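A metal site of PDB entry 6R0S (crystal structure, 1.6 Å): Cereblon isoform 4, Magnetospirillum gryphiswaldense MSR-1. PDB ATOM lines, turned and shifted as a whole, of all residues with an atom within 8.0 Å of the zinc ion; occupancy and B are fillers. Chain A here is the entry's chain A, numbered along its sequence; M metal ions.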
ATOM      1  N   ARG A  24       8.304  -1.873 -14.357  1.00  0.00           N
ATOM      2  CA  ARG A  24       8.422  -0.929 -13.262  1.00  0.00           C
ATOM      3  C   ARG A  24       9.821  -0.360 -13.170  1.00  0.00           C
ATOM      4  O   ARG A  24      10.769  -0.951 -13.657  1.00  0.00           O
ATOM      5  CB  ARG A  24       8.097  -1.650 -11.937  1.00  0.00           C
ATOM      6  CG  ARG A  24       6.689  -2.144 -11.874  1.00  0.00           C
ATOM      7  CD  ARG A  24       6.304  -2.714 -10.502  1.00  0.00           C
ATOM      8  NE  ARG A  24       4.888  -3.043 -10.546  1.00  0.00           N
ATOM      9  CZ  ARG A  24       3.889  -2.173 -10.427  1.00  0.00           C
ATOM     10  NH1 ARG A  24       4.102  -0.911 -10.121  1.00  0.00           N
ATOM     11  NH2 ARG A  24       2.651  -2.582 -10.562  1.00  0.00           N
ATOM     12  N   CYS A  25       9.973   0.798 -12.522  1.00  0.00           N
ATOM     13  CA  CYS A  25      11.276   1.325 -12.235  1.00  0.00           C
ATOM     14  C   CYS A  25      12.031   0.340 -11.339  1.00  0.00           C
ATOM     15  O   CYS A  25      11.488  -0.101 -10.311  1.00  0.00           O
ATOM     16  CB  CYS A  25      11.171   2.673 -11.561  1.00  0.00           C
ATOM     17  SG  CYS A  25      12.779   3.333 -10.992  1.00  0.00           S
ATOM     18  N   ARG A  26      13.234  -0.022 -11.746  1.00  0.00           N
ATOM     19  CA  ARG A  26      14.060  -0.947 -10.987  1.00  0.00           C
ATOM     20  C   ARG A  26      14.416  -0.470  -9.591  1.00  0.00           C
ATOM     21  O   ARG A  26      14.629  -1.285  -8.680  1.00  0.00           O
ATOM     22  CB  ARG A  26      15.324  -1.214 -11.784  1.00  0.00           C
ATOM     23  CG  ARG A  26      16.313  -2.099 -11.079  1.00  0.00           C
ATOM     24  CD  ARG A  26      17.442  -2.374 -12.018  1.00  0.00           C
ATOM     25  NE  ARG A  26      18.430  -3.104 -11.295  1.00  0.00           N
ATOM     26  CZ  ARG A  26      19.569  -3.538 -11.796  1.00  0.00           C
ATOM     27  NH1 ARG A  26      19.878  -3.323 -13.090  1.00  0.00           N
ATOM     28  NH2 ARG A  26      20.415  -4.184 -10.987  1.00  0.00           N
ATOM     29  N   GLN A  27      14.529   0.831  -9.418  1.00  0.00           N
ATOM     30  CA  GLN A  27      14.949   1.424  -8.129  1.00  0.00           C
ATOM     31  C   GLN A  27      13.832   1.550  -7.111  1.00  0.00           C
ATOM     32  O   GLN A  27      14.069   1.390  -5.925  1.00  0.00           O
ATOM     33  CB  GLN A  27      15.641   2.763  -8.354  1.00  0.00           C
ATOM     34  CG  GLN A  27      16.851   2.657  -9.257  1.00  0.00           C
ATOM     35  CD  GLN A  27      17.889   1.668  -8.753  1.00  0.00           C
ATOM     36  OE1 GLN A  27      18.156   1.577  -7.566  1.00  0.00           O
ATOM     37  NE2 GLN A  27      18.462   0.883  -9.673  1.00  0.00           N
ATOM     38  N   CYS A  28      12.612   1.816  -7.545  1.00  0.00           N
ATOM     39  CA  CYS A  28      11.523   2.138  -6.609  1.00  0.00           C
ATOM     40  C   CYS A  28      10.189   1.449  -6.893  1.00  0.00           C
ATOM     41  O   CYS A  28       9.273   1.530  -6.079  1.00  0.00           O
ATOM     42  CB  CYS A  28      11.343   3.643  -6.567  1.00  0.00           C
ATOM     43  SG  CYS A  28      10.501   4.264  -8.032  1.00  0.00           S
ATOM     44  N   GLY A  29      10.043   0.803  -8.046  1.00  0.00           N
ATOM     45  CA  GLY A  29       8.813   0.122  -8.359  1.00  0.00           C
ATOM     46  C   GLY A  29       7.700   0.900  -9.015  1.00  0.00           C
ATOM     47  O   GLY A  29       6.618   0.340  -9.309  1.00  0.00           O
ATOM     48  N   GLN A  30       7.916   2.195  -9.278  1.00  0.00           N
ATOM     49  CA  GLN A  30       6.896   2.971 -10.016  1.00  0.00           C
ATOM     50  C   GLN A  30       6.502   2.277 -11.312  1.00  0.00           C
ATOM     51  O   GLN A  30       7.337   1.804 -12.028  1.00  0.00           O
ATOM     52  CB  GLN A  30       7.526   4.327 -10.411  1.00  0.00           C
ATOM     53  CG  GLN A  30       6.693   5.213 -11.307  1.00  0.00           C
ATOM     54  CD  GLN A  30       5.788   6.129 -10.547  1.00  0.00           C
ATOM     55  OE1 GLN A  30       5.111   5.721  -9.628  1.00  0.00           O
ATOM     56  NE2 GLN A  30       5.772   7.410 -10.935  1.00  0.00           N
ATOM     57  N   THR A  31       5.202   2.232 -11.582  1.00  0.00           N
ATOM     58  CA  THR A  31       4.719   1.605 -12.815  1.00  0.00           C
ATOM     59  C   THR A  31       5.127   2.473 -13.995  1.00  0.00           C
ATOM     60  O   THR A  31       4.886   3.669 -13.945  1.00  0.00           O
ATOM     61  CB  THR A  31       3.173   1.484 -12.837  1.00  0.00           C
ATOM     62  OG1 THR A  31       2.684   0.994 -11.581  1.00  0.00           O
ATOM     63  CG2 THR A  31       2.767   0.615 -13.963  1.00  0.00           C
ATOM     64  N   ILE A  32       5.750   1.896 -15.018  1.00  0.00           N
ATOM     65  CA  ILE A  32       6.282   2.687 -16.150  1.00  0.00           C
ATOM     66  C   ILE A  32       5.684   2.283 -17.485  1.00  0.00           C
ATOM     67  O   ILE A  32       5.263   3.131 -18.227  1.00  0.00           O
ATOM     68  CB  ILE A  32       7.832   2.633 -16.273  1.00  0.00           C
ATOM     69  CG1 ILE A  32       8.533   3.083 -15.005  1.00  0.00           C
ATOM     70  CG2 ILE A  32       8.298   3.475 -17.465  1.00  0.00           C
ATOM     71  CD1 ILE A  32       8.289   4.517 -14.581  1.00  0.00           C
ATOM     72  N   GLY A  67       4.215   7.383 -15.394  1.00  0.00           N
ATOM     73  CA  GLY A  67       5.019   7.431 -14.184  1.00  0.00           C
ATOM     74  C   GLY A  67       6.363   8.113 -14.326  1.00  0.00           C
ATOM     75  O   GLY A  67       7.188   8.018 -13.431  1.00  0.00           O
ATOM     76  N   LEU A  68       6.602   8.757 -15.460  1.00  0.00           N
ATOM     77  CA  LEU A  68       7.848   9.442 -15.726  1.00  0.00           C
ATOM     78  C   LEU A  68       7.658  10.912 -15.479  1.00  0.00           C
ATOM     79  O   LEU A  68       6.538  11.379 -15.249  1.00  0.00           O
ATOM     80  CB  LEU A  68       8.299   9.216 -17.171  1.00  0.00           C
ATOM     81  CG  LEU A  68       8.575   7.762 -17.549  1.00  0.00           C
ATOM     82  CD1 LEU A  68       8.491   7.555 -19.058  1.00  0.00           C
ATOM     83  CD2 LEU A  68       9.889   7.270 -16.945  1.00  0.00           C
ATOM     84  N   LEU A  90      12.799  10.907 -16.527  1.00  0.00           N
ATOM     85  CA  LEU A  90      13.157  10.372 -15.218  1.00  0.00           C
ATOM     86  C   LEU A  90      11.975   9.619 -14.657  1.00  0.00           C
ATOM     87  O   LEU A  90      10.816   9.921 -14.976  1.00  0.00           O
ATOM     88  CB  LEU A  90      13.513  11.500 -14.279  1.00  0.00           C
ATOM     89  CG  LEU A  90      14.604  12.481 -14.733  1.00  0.00           C
ATOM     90  CD1 LEU A  90      14.858  13.492 -13.627  1.00  0.00           C
ATOM     91  CD2 LEU A  90      15.879  11.727 -15.103  1.00  0.00           C
ATOM     92  N   CYS A  91      12.254   8.654 -13.806  1.00  0.00           N
ATOM     93  CA  CYS A  91      11.205   8.096 -12.958  1.00  0.00           C
ATOM     94  C   CYS A  91      10.588   9.243 -12.164  1.00  0.00           C
ATOM     95  O   CYS A  91      11.280  10.015 -11.508  1.00  0.00           O
ATOM     96  CB  CYS A  91      11.777   7.093 -12.008  1.00  0.00           C
ATOM     97  SG  CYS A  91      10.529   6.384 -10.891  1.00  0.00           S
ATOM     98  N   GLY A  92       9.269   9.365 -12.258  1.00  0.00           N
ATOM     99  CA  GLY A  92       8.561  10.436 -11.596  1.00  0.00           C
ATOM    100  C   GLY A  92       8.549  10.296 -10.112  1.00  0.00           C
ATOM    101  O   GLY A  92       8.297  11.285  -9.425  1.00  0.00           O
ATOM    102  N   GLN A  93       8.780   9.090  -9.619  1.00  0.00           N
ATOM    103  CA  GLN A  93       8.769   8.805  -8.195  1.00  0.00           C
ATOM    104  C   GLN A  93      10.156   9.063  -7.610  1.00  0.00           C
ATOM    105  O   GLN A  93      10.291   9.847  -6.685  1.00  0.00           O
ATOM    106  CB  GLN A  93       8.282   7.386  -7.977  1.00  0.00           C
ATOM    107  CG  GLN A  93       8.139   7.009  -6.508  1.00  0.00           C
ATOM    108  CD  GLN A  93       7.185   5.837  -6.323  1.00  0.00           C
ATOM    109  OE1 GLN A  93       6.022   6.063  -6.059  1.00  0.00           O
ATOM    110  NE2 GLN A  93       7.654   4.618  -6.532  1.00  0.00           N
ATOM    111  N   CYS A  94      11.183   8.398  -8.141  1.00  0.00           N
ATOM    112  CA  CYS A  94      12.518   8.450  -7.517  1.00  0.00           C
ATOM    113  C   CYS A  94      13.614   9.237  -8.242  1.00  0.00           C
ATOM    114  O   CYS A  94      14.690   9.429  -7.673  1.00  0.00           O
ATOM    115  CB  CYS A  94      13.012   7.042  -7.282  1.00  0.00           C
ATOM    116  SG  CYS A  94      13.727   6.197  -8.732  1.00  0.00           S
ATOM    117  N   GLY A  95      13.327   9.681  -9.466  1.00  0.00           N
ATOM    118  CA  GLY A  95      14.284  10.468 -10.225  1.00  0.00           C
ATOM    119  C   GLY A  95      15.309   9.686 -11.018  1.00  0.00           C
ATOM    120  O   GLY A  95      16.136  10.291 -11.688  1.00  0.00           O
ATOM    121  N   SER A  96      15.279   8.355 -10.973  1.00  0.00           N
ATOM    122  CA  SER A  96      16.177   7.506 -11.774  1.00  0.00           C
ATOM    123  C   SER A  96      16.024   7.851 -13.258  1.00  0.00           C
ATOM    124  O   SER A  96      14.914   8.026 -13.737  1.00  0.00           O
ATOM    125  CB  SER A  96      15.867   6.030 -11.568  1.00  0.00           C
ATOM    126  OG  SER A  96      16.705   5.178 -12.358  1.00  0.00           O
ATOM    127  N   HIS A  97      17.137   7.960 -13.973  1.00  0.00           N
ATOM    128  CA  HIS A  97      17.036   8.247 -15.396  1.00  0.00           C
ATOM    129  C   HIS A  97      16.667   6.986 -16.150  1.00  0.00           C
ATOM    130  O   HIS A  97      17.478   6.067 -16.259  1.00  0.00           O
ATOM    131  CB  HIS A  97      18.360   8.807 -15.904  1.00  0.00           C
ATOM    132  CG  HIS A  97      18.340   9.082 -17.359  1.00  0.00           C
ATOM    133  ND1 HIS A  97      19.492   9.084 -18.114  1.00  0.00           N
ATOM    134  CD2 HIS A  97      17.306   9.326 -18.198  1.00  0.00           C
ATOM    135  CE1 HIS A  97      19.163   9.335 -19.364  1.00  0.00           C
ATOM    136  NE2 HIS A  97      17.855   9.484 -19.452  1.00  0.00           N
ATOM    137  N   LEU A  98      15.422   6.916 -16.638  1.00  0.00           N
ATOM    138  CA  LEU A  98      14.923   5.693 -17.272  1.00  0.00           C
ATOM    139  C   LEU A  98      15.010   5.687 -18.788  1.00  0.00           C
ATOM    140  O   LEU A  98      14.946   4.633 -19.408  1.00  0.00           O
ATOM    141  CB  LEU A  98      13.492   5.410 -16.846  1.00  0.00           C
ATOM    142  CG  LEU A  98      13.322   5.133 -15.340  1.00  0.00           C
ATOM    143  CD1 LEU A  98      11.901   4.690 -15.070  1.00  0.00           C
ATOM    144  CD2 LEU A  98      14.298   4.089 -14.788  1.00  0.00           C
ATOM    145  N   ARG A 118      17.273  -0.657 -16.595  1.00  0.00           N
ATOM    146  CA  ARG A 118      16.809   0.203 -15.535  1.00  0.00           C
ATOM    147  C   ARG A 118      15.348  -0.038 -15.176  1.00  0.00           C
ATOM    148  O   ARG A 118      14.774   0.667 -14.321  1.00  0.00           O
ATOM    149  CB  ARG A 118      17.072   1.665 -15.904  1.00  0.00           C
ATOM    150  CG  ARG A 118      18.568   1.909 -16.051  1.00  0.00           C
ATOM    151  CD  ARG A 118      18.944   3.344 -16.265  1.00  0.00           C
ATOM    152  NE  ARG A 118      20.351   3.473 -16.606  1.00  0.00           N
ATOM    153  CZ  ARG A 118      20.989   4.634 -16.761  1.00  0.00           C
ATOM    154  NH1 ARG A 118      20.363   5.811 -16.580  1.00  0.00           N
ATOM    155  NH2 ARG A 118      22.296   4.646 -17.036  1.00  0.00           N
HETATM  156 ZN    ZN M   1      11.962   5.005  -9.642  1.00  0.00          ZN
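N of Gln 30 sits close to SG of Cys 28 (3.5 Å).
SG of Cys 28 sits close to NE2 of Gln 93 (3.2 Å).
SG of Cys 25 lies close to N of Gln 27 (3.4 Å).
The backbone NH (N) of Cys 25 lies within hydrogen-bond range of the backbone carbonyl oxygen (O) of Gln 30 (2.9 Å).
The backbone NH (N) of Ser 96 sits close to the side-chain sulfur (SG) of Cys 94 (3.5 Å).
N of Cys 91 lies within hydrogen-bond range of O of Ser 96.
The side-chain sulfur of Cys 91 lies close to the backbone NH of Gln 93, at 3.5 Å.
The nearest printed residue that does not touch the zinc ion is Ser 96 (4.5 Å).
The zinc ion is bound by the side-chain sulfur (SG) of Cys 28 (2.3 Å), the side-chain sulfur (SG) of Cys 25 (2.3 Å), the side-chain sulfur (SG) of Cys 94 (2.3 Å) and the side-chain sulfur (SG) of Cys 91 (2.3 Å).
The zinc ion has four donor atoms within binding distance.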
